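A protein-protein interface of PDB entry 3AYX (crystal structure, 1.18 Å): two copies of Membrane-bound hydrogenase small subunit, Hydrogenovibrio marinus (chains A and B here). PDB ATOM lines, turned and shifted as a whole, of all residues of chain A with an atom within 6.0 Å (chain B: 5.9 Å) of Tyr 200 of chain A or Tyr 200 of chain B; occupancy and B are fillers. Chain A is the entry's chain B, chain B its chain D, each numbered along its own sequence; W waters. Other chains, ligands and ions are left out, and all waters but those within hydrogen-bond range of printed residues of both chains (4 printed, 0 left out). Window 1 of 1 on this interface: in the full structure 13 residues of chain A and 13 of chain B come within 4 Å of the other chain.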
ATOM      1  N   ASP A 197     -36.350 -23.889   5.332  1.00  0.00           N
ATOM      2  CA  ASP A 197     -35.833 -23.660   3.977  1.00  0.00           C
ATOM      3  C   ASP A 197     -34.367 -23.348   3.990  1.00  0.00           C
ATOM      4  O   ASP A 197     -33.790 -23.272   2.893  1.00  0.00           O
ATOM      5  CB  ASP A 197     -36.612 -22.478   3.358  1.00  0.00           C
ATOM      6  CG  ASP A 197     -38.020 -22.660   3.013  1.00  0.00           C
ATOM      7  OD1 ASP A 197     -38.438 -23.785   2.724  1.00  0.00           O
ATOM      8  OD2 ASP A 197     -38.807 -21.697   3.054  1.00  0.00           O
ATOM      9  N   LYS A 198     -33.738 -23.112   5.129  1.00  0.00           N
ATOM     10  CA  LYS A 198     -32.340 -22.742   5.249  1.00  0.00           C
ATOM     11  C   LYS A 198     -31.720 -23.378   6.482  1.00  0.00           C
ATOM     12  O   LYS A 198     -30.785 -22.836   7.082  1.00  0.00           O
ATOM     13  CB  LYS A 198     -32.149 -21.215   5.223  1.00  0.00           C
ATOM     14  CG  LYS A 198     -32.353 -20.495   3.855  1.00  0.00           C
ATOM     15  CD  LYS A 198     -31.329 -20.979   2.823  1.00  0.00           C
ATOM     16  CE  LYS A 198     -30.752 -20.076   1.773  1.00  0.00           C
ATOM     17  NZ  LYS A 198     -31.829 -19.503   0.888  1.00  0.00           N
ATOM     18  N   CYS A 199     -32.186 -24.517   6.953  1.00  0.00           N
ATOM     19  CA  CYS A 199     -31.731 -25.111   8.224  1.00  0.00           C
ATOM     20  C   CYS A 199     -30.618 -26.084   8.000  1.00  0.00           C
ATOM     21  O   CYS A 199     -30.735 -27.048   7.226  1.00  0.00           O
ATOM     22  CB  CYS A 199     -32.926 -25.850   8.879  1.00  0.00           C
ATOM     23  SG  CYS A 199     -32.440 -26.479  10.528  1.00  0.00           S
ATOM     24  N   TYR A 200     -29.534 -25.871   8.701  1.00  0.00           N
ATOM     25  CA  TYR A 200     -28.331 -26.717   8.639  1.00  0.00           C
ATOM     26  C   TYR A 200     -28.578 -28.129   9.171  1.00  0.00           C
ATOM     27  O   TYR A 200     -27.746 -28.970   8.853  1.00  0.00           O
ATOM     28  CB  TYR A 200     -27.153 -26.011   9.388  1.00  0.00           C
ATOM     29  CG  TYR A 200     -27.212 -26.285  10.873  1.00  0.00           C
ATOM     30  CD1 TYR A 200     -26.347 -27.161  11.492  1.00  0.00           C
ATOM     31  CD2 TYR A 200     -28.175 -25.703  11.698  1.00  0.00           C
ATOM     32  CE1 TYR A 200     -26.344 -27.457  12.845  1.00  0.00           C
ATOM     33  CE2 TYR A 200     -28.236 -26.018  13.034  1.00  0.00           C
ATOM     34  CZ  TYR A 200     -27.346 -26.867  13.609  1.00  0.00           C
ATOM     35  OH  TYR A 200     -27.513 -27.177  14.949  1.00  0.00           O
ATOM     36  N   ARG A 201     -29.679 -28.392   9.865  1.00  0.00           N
ATOM     37  CA  ARG A 201     -30.023 -29.780  10.256  1.00  0.00           C
ATOM     38  C   ARG A 201     -30.834 -30.504   9.185  1.00  0.00           C
ATOM     39  O   ARG A 201     -31.111 -31.693   9.320  1.00  0.00           O
ATOM     40  CB  ARG A 201     -30.707 -29.899  11.611  1.00  0.00           C
ATOM     41  CG  ARG A 201     -29.884 -29.331  12.752  1.00  0.00           C
ATOM     42  CD  ARG A 201     -30.495 -29.753  14.090  1.00  0.00           C
ATOM     43  NE  ARG A 201     -29.688 -29.211  15.216  1.00  0.00           N
ATOM     44  CZ  ARG A 201     -29.623 -29.714  16.436  1.00  0.00           C
ATOM     45  NH1 ARG A 201     -28.860 -29.104  17.356  1.00  0.00           N
ATOM     46  NH2 ARG A 201     -30.259 -30.797  16.768  1.00  0.00           N
ATOM     47  N   ARG A 202     -31.184 -29.817   8.092  1.00  0.00           N
ATOM     48  CA  ARG A 202     -31.940 -30.435   7.012  1.00  0.00           C
ATOM     49  C   ARG A 202     -31.328 -31.731   6.482  1.00  0.00           C
ATOM     50  O   ARG A 202     -32.097 -32.656   6.182  1.00  0.00           O
ATOM     51  CB  ARG A 202     -32.186 -29.492   5.865  1.00  0.00           C
ATOM     52  CG  ARG A 202     -33.054 -30.017   4.737  1.00  0.00           C
ATOM     53  CD  ARG A 202     -34.526 -30.205   5.239  1.00  0.00           C
ATOM     54  NE  ARG A 202     -35.248 -30.546   3.994  1.00  0.00           N
ATOM     55  CZ  ARG A 202     -35.924 -29.734   3.194  1.00  0.00           C
ATOM     56  NH1 ARG A 202     -36.071 -28.437   3.553  1.00  0.00           N
ATOM     57  NH2 ARG A 202     -36.425 -30.267   2.144  1.00  0.00           N
ATOM     58  N   PRO A 203     -29.998 -31.863   6.316  1.00  0.00           N
ATOM     59  CA  PRO A 203     -29.479 -33.184   5.864  1.00  0.00           C
ATOM     60  C   PRO A 203     -29.953 -34.336   6.724  1.00  0.00           C
ATOM     61  O   PRO A 203     -30.255 -35.420   6.201  1.00  0.00           O
ATOM     62  CB  PRO A 203     -27.977 -33.000   5.980  1.00  0.00           C
ATOM     63  CG  PRO A 203     -27.792 -31.492   5.766  1.00  0.00           C
ATOM     64  CD  PRO A 203     -28.911 -30.887   6.482  1.00  0.00           C
ATOM     65  N   HIS A 204     -30.118 -34.159   8.019  1.00  0.00           N
ATOM     66  CA  HIS A 204     -30.621 -35.158   8.923  1.00  0.00           C
ATOM     67  C   HIS A 204     -32.087 -35.393   8.690  1.00  0.00           C
ATOM     68  O   HIS A 204     -32.509 -36.551   8.608  1.00  0.00           O
ATOM     69  CB  HIS A 204     -30.308 -34.822  10.371  1.00  0.00           C
ATOM     70  CG  HIS A 204     -28.846 -34.762  10.638  1.00  0.00           C
ATOM     71  ND1 HIS A 204     -28.001 -35.816  10.436  1.00  0.00           N
ATOM     72  CD2 HIS A 204     -28.040 -33.780  11.100  1.00  0.00           C
ATOM     73  CE1 HIS A 204     -26.804 -35.459  10.777  1.00  0.00           C
ATOM     74  NE2 HIS A 204     -26.757 -34.203  11.174  1.00  0.00           N
ATOM     75  N   GLY A 222     -26.609 -33.579  16.753  1.00  0.00           N
ATOM     76  CA  GLY A 222     -27.325 -32.490  16.050  1.00  0.00           C
ATOM     77  C   GLY A 222     -28.307 -32.933  15.033  1.00  0.00           C
ATOM     78  O   GLY A 222     -28.510 -32.224  14.031  1.00  0.00           O
ATOM     79  N   SER A 240     -32.356 -19.079  10.792  1.00  0.00           N
ATOM     80  CA  SER A 240     -31.418 -20.071  10.258  1.00  0.00           C
ATOM     81  C   SER A 240     -30.384 -19.472   9.321  1.00  0.00           C
ATOM     82  O   SER A 240     -29.518 -20.178   8.864  1.00  0.00           O
ATOM     83  CB  SER A 240     -32.179 -21.249   9.695  1.00  0.00           C
ATOM     84  OG  SER A 240     -33.132 -20.785   8.723  1.00  0.00           O
ATOM     85  N   THR A 241     -30.431 -18.140   9.054  1.00  0.00           N
ATOM     86  CA  THR A 241     -29.570 -17.470   8.105  1.00  0.00           C
ATOM     87  C   THR A 241     -28.782 -16.380   8.848  1.00  0.00           C
ATOM     88  O   THR A 241     -27.562 -16.400   8.883  1.00  0.00           O
ATOM     89  CB  THR A 241     -30.400 -16.843   6.915  1.00  0.00           C
ATOM     90  OG1 THR A 241     -31.588 -16.226   7.413  1.00  0.00           O
ATOM     91  CG2 THR A 241     -30.757 -17.991   5.957  1.00  0.00           C
ATOM     92  N   PHE A 250     -29.088 -20.081  17.213  1.00  0.00           N
ATOM     93  CA  PHE A 250     -30.534 -19.919  17.078  1.00  0.00           C
ATOM     94  C   PHE A 250     -31.159 -21.133  17.818  1.00  0.00           C
ATOM     95  O   PHE A 250     -30.449 -22.047  18.203  1.00  0.00           O
ATOM     96  CB  PHE A 250     -30.976 -19.773  15.648  1.00  0.00           C
ATOM     97  CG  PHE A 250     -30.938 -20.932  14.711  1.00  0.00           C
ATOM     98  CD1 PHE A 250     -32.055 -21.492  14.135  1.00  0.00           C
ATOM     99  CD2 PHE A 250     -29.726 -21.478  14.294  1.00  0.00           C
ATOM    100  CE1 PHE A 250     -32.060 -22.455  13.183  1.00  0.00           C
ATOM    101  CE2 PHE A 250     -29.687 -22.489  13.325  1.00  0.00           C
ATOM    102  CZ  PHE A 250     -30.842 -23.013  12.768  1.00  0.00           C
ATOM    103  N   ILE A 252     -32.698 -23.931  17.203  1.00  0.00           N
ATOM    104  CA  ILE A 252     -32.379 -25.246  16.696  1.00  0.00           C
ATOM    105  C   ILE A 252     -30.909 -25.570  16.923  1.00  0.00           C
ATOM    106  O   ILE A 252     -30.588 -26.700  17.310  1.00  0.00           O
ATOM    107  CB  ILE A 252     -32.794 -25.330  15.211  1.00  0.00           C
ATOM    108  CG1 ILE A 252     -34.326 -25.360  15.111  1.00  0.00           C
ATOM    109  CG2 ILE A 252     -32.104 -26.484  14.491  1.00  0.00           C
ATOM    110  CD1 ILE A 252     -34.897 -24.647  13.956  1.00  0.00           C
ATOM    111  N   GLN A 253     -30.000 -24.636  16.685  1.00  0.00           N
ATOM    112  CA  GLN A 253     -28.601 -24.931  16.942  1.00  0.00           C
ATOM    113  C   GLN A 253     -28.365 -25.369  18.384  1.00  0.00           C
ATOM    114  O   GLN A 253     -27.613 -26.295  18.630  1.00  0.00           O
ATOM    115  CB  GLN A 253     -27.715 -23.736  16.585  1.00  0.00           C
ATOM    116  CG  GLN A 253     -26.248 -24.023  16.872  1.00  0.00           C
ATOM    117  CD  GLN A 253     -25.324 -22.914  16.409  1.00  0.00           C
ATOM    118  OE1 GLN A 253     -25.706 -21.994  15.712  1.00  0.00           O
ATOM    119  NE2 GLN A 253     -24.056 -23.076  16.792  1.00  0.00           N
ATOM    120  N   SER A 254     -29.023 -24.726  19.328  1.00  0.00           N
ATOM    121  CA  SER A 254     -28.881 -25.021  20.746  1.00  0.00           C
ATOM    122  C   SER A 254     -29.753 -26.152  21.202  1.00  0.00           C
ATOM    123  O   SER A 254     -29.688 -26.522  22.387  1.00  0.00           O
ATOM    124  CB  SER A 254     -29.193 -23.761  21.518  1.00  0.00           C
ATOM    125  OG  SER A 254     -28.222 -22.740  21.257  1.00  0.00           O
ATOM    126  N   ASP B 197     -23.294 -32.545   5.093  1.00  0.00           N
ATOM    127  CA  ASP B 197     -24.080 -33.183   6.156  1.00  0.00           C
ATOM    128  C   ASP B 197     -24.663 -32.202   7.149  1.00  0.00           C
ATOM    129  O   ASP B 197     -25.502 -32.580   7.929  1.00  0.00           O
ATOM    130  CB  ASP B 197     -23.184 -34.134   6.923  1.00  0.00           C
ATOM    131  CG  ASP B 197     -22.703 -35.360   6.174  1.00  0.00           C
ATOM    132  OD1 ASP B 197     -23.371 -35.828   5.254  1.00  0.00           O
ATOM    133  OD2 ASP B 197     -21.614 -35.861   6.592  1.00  0.00           O
ATOM    134  N   LYS B 198     -24.242 -30.914   7.057  1.00  0.00           N
ATOM    135  CA  LYS B 198     -24.739 -29.857   7.935  1.00  0.00           C
ATOM    136  C   LYS B 198     -24.876 -28.527   7.171  1.00  0.00           C
ATOM    137  O   LYS B 198     -24.723 -27.465   7.759  1.00  0.00           O
ATOM    138  CB  LYS B 198     -23.803 -29.722   9.139  1.00  0.00           C
ATOM    139  CG  LYS B 198     -23.932 -30.896  10.192  1.00  0.00           C
ATOM    140  CD  LYS B 198     -25.339 -30.951  10.784  1.00  0.00           C
ATOM    141  CE  LYS B 198     -25.447 -31.285  12.304  1.00  0.00           C
ATOM    142  NZ  LYS B 198     -24.946 -32.686  12.585  1.00  0.00           N
ATOM    143  N   CYS B 199     -25.162 -28.532   5.894  1.00  0.00           N
ATOM    144  CA  CYS B 199     -25.155 -27.345   5.085  1.00  0.00           C
ATOM    145  C   CYS B 199     -26.525 -26.712   5.030  1.00  0.00           C
ATOM    146  O   CYS B 199     -27.544 -27.352   4.575  1.00  0.00           O
ATOM    147  CB  CYS B 199     -24.716 -27.717   3.618  1.00  0.00           C
ATOM    148  SG  CYS B 199     -24.589 -26.116   2.652  1.00  0.00           S
ATOM    149  N   TYR B 200     -26.634 -25.440   5.395  1.00  0.00           N
ATOM    150  CA  TYR B 200     -27.885 -24.683   5.402  1.00  0.00           C
ATOM    151  C   TYR B 200     -28.510 -24.474   3.993  1.00  0.00           C
ATOM    152  O   TYR B 200     -29.677 -24.148   3.904  1.00  0.00           O
ATOM    153  CB  TYR B 200     -27.670 -23.341   6.137  1.00  0.00           C
ATOM    154  CG  TYR B 200     -27.088 -22.300   5.232  1.00  0.00           C
ATOM    155  CD1 TYR B 200     -27.851 -21.247   4.731  1.00  0.00           C
ATOM    156  CD2 TYR B 200     -25.786 -22.327   4.774  1.00  0.00           C
ATOM    157  CE1 TYR B 200     -27.338 -20.293   3.878  1.00  0.00           C
ATOM    158  CE2 TYR B 200     -25.254 -21.447   3.912  1.00  0.00           C
ATOM    159  CZ  TYR B 200     -26.038 -20.415   3.466  1.00  0.00           C
ATOM    160  OH  TYR B 200     -25.597 -19.480   2.579  1.00  0.00           O
ATOM    161  N   ARG B 201     -27.719 -24.707   2.927  1.00  0.00           N
ATOM    162  CA  ARG B 201     -28.321 -24.656   1.575  1.00  0.00           C
ATOM    163  C   ARG B 201     -28.904 -25.992   1.149  1.00  0.00           C
ATOM    164  O   ARG B 201     -29.471 -26.122   0.062  1.00  0.00           O
ATOM    165  CB  ARG B 201     -27.316 -24.160   0.537  1.00  0.00           C
ATOM    166  CG  ARG B 201     -26.821 -22.743   0.806  1.00  0.00           C
ATOM    167  CD  ARG B 201     -26.104 -22.170  -0.426  1.00  0.00           C
ATOM    168  NE  ARG B 201     -25.627 -20.841  -0.210  1.00  0.00           N
ATOM    169  CZ  ARG B 201     -25.383 -19.881  -1.087  1.00  0.00           C
ATOM    170  NH1 ARG B 201     -25.603 -20.099  -2.356  1.00  0.00           N
ATOM    171  NH2 ARG B 201     -24.922 -18.695  -0.685  1.00  0.00           N
ATOM    172  N   ARG B 202     -28.795 -27.022   2.000  1.00  0.00           N
ATOM    173  CA  ARG B 202     -29.328 -28.353   1.664  1.00  0.00           C
ATOM    174  C   ARG B 202     -30.837 -28.288   1.254  1.00  0.00           C
ATOM    175  O   ARG B 202     -31.186 -29.072   0.321  1.00  0.00           O
ATOM    176  CB  ARG B 202     -29.094 -29.325   2.800  1.00  0.00           C
ATOM    177  CG  ARG B 202     -29.540 -30.759   2.520  1.00  0.00           C
ATOM    178  CD  ARG B 202     -28.729 -31.410   1.342  1.00  0.00           C
ATOM    179  NE  ARG B 202     -29.252 -32.777   1.305  1.00  0.00           N
ATOM    180  CZ  ARG B 202     -28.654 -33.768   1.968  1.00  0.00           C
ATOM    181  NH1 ARG B 202     -29.228 -34.934   1.929  1.00  0.00           N
ATOM    182  NH2 ARG B 202     -27.501 -33.678   2.670  1.00  0.00           N
ATOM    183  N   PRO B 203     -31.692 -27.495   1.859  1.00  0.00           N
ATOM    184  CA  PRO B 203     -33.123 -27.450   1.395  1.00  0.00           C
ATOM    185  C   PRO B 203     -33.214 -27.183  -0.093  1.00  0.00           C
ATOM    186  O   PRO B 203     -34.061 -27.753  -0.804  1.00  0.00           O
ATOM    187  CB  PRO B 203     -33.741 -26.374   2.267  1.00  0.00           C
ATOM    188  CG  PRO B 203     -32.932 -26.438   3.539  1.00  0.00           C
ATOM    189  CD  PRO B 203     -31.526 -26.654   3.068  1.00  0.00           C
ATOM    190  N   HIS B 204     -32.327 -26.339  -0.615  1.00  0.00           N
ATOM    191  CA  HIS B 204     -32.295 -26.064  -2.042  1.00  0.00           C
ATOM    192  C   HIS B 204     -31.762 -27.202  -2.858  1.00  0.00           C
ATOM    193  O   HIS B 204     -32.385 -27.528  -3.871  1.00  0.00           O
ATOM    194  CB  HIS B 204     -31.493 -24.746  -2.280  1.00  0.00           C
ATOM    195  CG  HIS B 204     -32.152 -23.575  -1.651  1.00  0.00           C
ATOM    196  ND1 HIS B 204     -33.401 -23.137  -1.942  1.00  0.00           N
ATOM    197  CD2 HIS B 204     -31.681 -22.671  -0.740  1.00  0.00           C
ATOM    198  CE1 HIS B 204     -33.650 -22.027  -1.214  1.00  0.00           C
ATOM    199  NE2 HIS B 204     -32.615 -21.728  -0.460  1.00  0.00           N
ATOM    200  N   GLY B 222     -29.454 -17.609  -2.533  1.00  0.00           N
ATOM    201  CA  GLY B 222     -28.684 -18.583  -1.782  1.00  0.00           C
ATOM    202  C   GLY B 222     -28.963 -20.017  -2.096  1.00  0.00           C
ATOM    203  O   GLY B 222     -28.866 -20.901  -1.244  1.00  0.00           O
ATOM    204  N   SER B 240     -19.470 -25.767   8.058  1.00  0.00           N
ATOM    205  CA  SER B 240     -20.906 -25.549   8.060  1.00  0.00           C
ATOM    206  C   SER B 240     -21.542 -25.531   9.431  1.00  0.00           C
ATOM    207  O   SER B 240     -22.742 -25.298   9.569  1.00  0.00           O
ATOM    208  CB  SER B 240     -21.573 -26.513   7.068  1.00  0.00           C
ATOM    209  OG  SER B 240     -21.239 -27.874   7.343  1.00  0.00           O
ATOM    210  N   THR B 241     -20.738 -25.773  10.483  1.00  0.00           N
ATOM    211  CA  THR B 241     -21.177 -25.868  11.842  1.00  0.00           C
ATOM    212  C   THR B 241     -20.493 -24.805  12.688  1.00  0.00           C
ATOM    213  O   THR B 241     -21.193 -23.919  13.269  1.00  0.00           O
ATOM    214  CB  THR B 241     -20.935 -27.308  12.433  1.00  0.00           C
ATOM    215  OG1 THR B 241     -19.614 -27.757  12.055  1.00  0.00           O
ATOM    216  CG2 THR B 241     -21.999 -28.257  11.899  1.00  0.00           C
ATOM    217  N   PHE B 250     -18.740 -18.882   5.876  1.00  0.00           N
ATOM    218  CA  PHE B 250     -17.892 -19.962   5.362  1.00  0.00           C
ATOM    219  C   PHE B 250     -18.019 -19.878   3.825  1.00  0.00           C
ATOM    220  O   PHE B 250     -18.874 -19.096   3.316  1.00  0.00           O
ATOM    221  CB  PHE B 250     -18.252 -21.338   5.889  1.00  0.00           C
ATOM    222  CG  PHE B 250     -19.558 -21.989   5.529  1.00  0.00           C
ATOM    223  CD1 PHE B 250     -19.605 -23.177   4.822  1.00  0.00           C
ATOM    224  CD2 PHE B 250     -20.760 -21.440   5.949  1.00  0.00           C
ATOM    225  CE1 PHE B 250     -20.756 -23.861   4.515  1.00  0.00           C
ATOM    226  CE2 PHE B 250     -21.959 -22.136   5.647  1.00  0.00           C
ATOM    227  CZ  PHE B 250     -21.955 -23.343   4.955  1.00  0.00           C
ATOM    228  N   ILE B 252     -19.404 -21.382   1.309  1.00  0.00           N
ATOM    229  CA  ILE B 252     -20.730 -21.541   0.708  1.00  0.00           C
ATOM    230  C   ILE B 252     -21.623 -20.413   1.109  1.00  0.00           C
ATOM    231  O   ILE B 252     -22.380 -19.887   0.257  1.00  0.00           O
ATOM    232  CB  ILE B 252     -21.288 -22.929   1.106  1.00  0.00           C
ATOM    233  CG1 ILE B 252     -20.589 -24.054   0.322  1.00  0.00           C
ATOM    234  CG2 ILE B 252     -22.776 -23.000   0.936  1.00  0.00           C
ATOM    235  CD1 ILE B 252     -20.374 -25.283   1.100  1.00  0.00           C
ATOM    236  N   GLN B 253     -21.575 -19.924   2.363  1.00  0.00           N
ATOM    237  CA  GLN B 253     -22.390 -18.784   2.726  1.00  0.00           C
ATOM    238  C   GLN B 253     -22.160 -17.599   1.856  1.00  0.00           C
ATOM    239  O   GLN B 253     -23.077 -16.902   1.424  1.00  0.00           O
ATOM    240  CB  GLN B 253     -22.271 -18.455   4.228  1.00  0.00           C
ATOM    241  CG  GLN B 253     -23.137 -17.265   4.584  1.00  0.00           C
ATOM    242  CD  GLN B 253     -23.112 -16.956   6.078  1.00  0.00           C
ATOM    243  OE1 GLN B 253     -22.606 -17.693   6.877  1.00  0.00           O
ATOM    244  NE2 GLN B 253     -23.694 -15.788   6.402  1.00  0.00           N
ATOM    245  N   SER B 254     -20.899 -17.349   1.554  1.00  0.00           N
ATOM    246  CA  SER B 254     -20.493 -16.216   0.778  1.00  0.00           C
ATOM    247  C   SER B 254     -20.551 -16.436  -0.700  1.00  0.00           C
ATOM    248  O   SER B 254     -20.232 -15.550  -1.510  1.00  0.00           O
ATOM    249  CB  SER B 254     -19.084 -15.788   1.158  1.00  0.00           C
ATOM    250  OG  SER B 254     -19.027 -15.345   2.520  1.00  0.00           O
HETATM  251  O   HOH W   1     -36.656 -28.422  -0.047  1.00  0.00           O
HETATM  252  O   HOH W   2     -28.917 -36.684   4.139  1.00  0.00           O
HETATM  253  O   HOH W   3     -25.252 -14.682   8.759  1.00  0.00           O
HETATM  254  O   HOH W   4     -21.316 -22.504  15.767  1.00  0.00           O
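O of Asp 197 of chain A touches CB of Pro 203 of chain B, at 3.2 Å. Tyr 200 of chain B touches Lys 198 of chain A (CB to O, 3.3 Å). Lys 198 of chain A touches Gly 222 of chain B. Tyr 200 of chain B touches Cys 199 of chain A (O to N, 3.97 Å). Cys 199 of chain A touches Pro 203 of chain B (N to CG, 3.99 Å). O of Tyr 200 of chain A touches CA of Lys 198 of chain B (3.3 Å). Tyr 200 of chain A touches Tyr 200 of chain B (CA to CA, 3.8 Å). Asp 197 of chain B touches Pro 203 of chain A. CG of Pro 203 of chain A touches N of Lys 198 of chain B (3.8 Å). His 204 of chain A touches Asp 197 of chain B (NE2 to O, 3.8 Å).
O of Gly 222 of chain B lies close to NE of Arg 201 of chain B (3.4 Å). The side-chain sulfur of Cys 199 of chain B sits close to the backbone NH of Arg 201 of chain B (3.4 Å). NE of Arg 201 of chain A sits at hydrogen-bond distance from OH of Tyr 200 of chain A, at 3.0 Å. The side-chain hydroxyl (OH) of Tyr 200 of chain B is in hydrogen-bond range of the guanidinium group (NE) of Arg 201 of chain B (3.1 Å). NE of Arg 201 of chain A sits close to O of Gly 222 of chain A, at 3.4 Å. SG of Cys 199 of chain A sits close to N of Arg 201 of chain A.
Hydrophobic or aromatic side chains of chain A within 4 Å of the printed part of chain B: Tyr 200, Pro 203 and His 204.
Asp 197 of chain A touches His 204 of chain B, and with the chains exchanged His 204 of chain A touches Asp 197 of chain B. Lys 198 of chain A touches Tyr 200 of chain B, and with the chains exchanged Tyr 200 of chain A touches Lys 198 of chain B. Lys 198 of chain A touches Pro 203 of chain B, and with the chains exchanged Pro 203 of chain A touches Lys 198 of chain B. Lys 198 of chain A touches Gly 222 of chain B, and with the chains exchanged Gly 222 of chain A touches Lys 198 of chain B. Positions printed for both chains: 197, 198, 199, 200, 201, 202, 203, 204, 222, 240, 241, 250, 252, 253 and 254. Of the 19 pairs that touch across the chains among the printed residues, 19 have their exchanged pair printed and touching as well.
The side-chain amino group (NZ) of Lys 198 of chain A sits at hydrogen-bond distance from a ring nitrogen (NE2) of His 204 of chain B, at 2.7 Å. A ring nitrogen (NE2) of His 204 of chain A sits at hydrogen-bond distance from the side-chain amino group (NZ) of Lys 198 of chain B, 2.8 Å away.
Water W2 lies within hydrogen-bond range of O of Pro 203 of chain A and NH1 of Arg 202 of chain B. Water W1 bridges the backbone carbonyl oxygen (O) of Pro 203 of chain B and the guanidinium group (NH2) of Arg 202 of chain A. Water W4 lies within hydrogen-bond range of the backbone carbonyl oxygen of Thr 241 of chain B (2.9 Å) and the side-chain amide nitrogen of Gln 253 of chain A (3.0 Å). Water W3 lies within hydrogen-bond range of the backbone carbonyl oxygen of Thr 241 of chain A (2.9 Å) and the side-chain amide nitrogen of Gln 253 of chain B (3.0 Å).
Of chain A, only Lys 198 (3.3 Å), Cys 199 (3.97 Å) and Tyr 200 (3.8 Å) come within 4 Å of Tyr 200 of chain B. Printed residues of chain B within 4 Å of Lys 198 of chain A: Tyr 200, Pro 203, His 204 and Gly 222. Of the printed residues of chain B, Gly 222 of chain A touches Lys 198 (3.6 Å). Of the printed residues of chain A, Gly 222 of chain B touches Lys 198 (3.7 Å). Of the printed residues of chain A, Cys 199 of chain B touches Tyr 200 and Pro 203. Ser 254 of chain A touches none of the printed residues of chain B. Ser 240 of chain B touches none of the printed residues of chain A.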
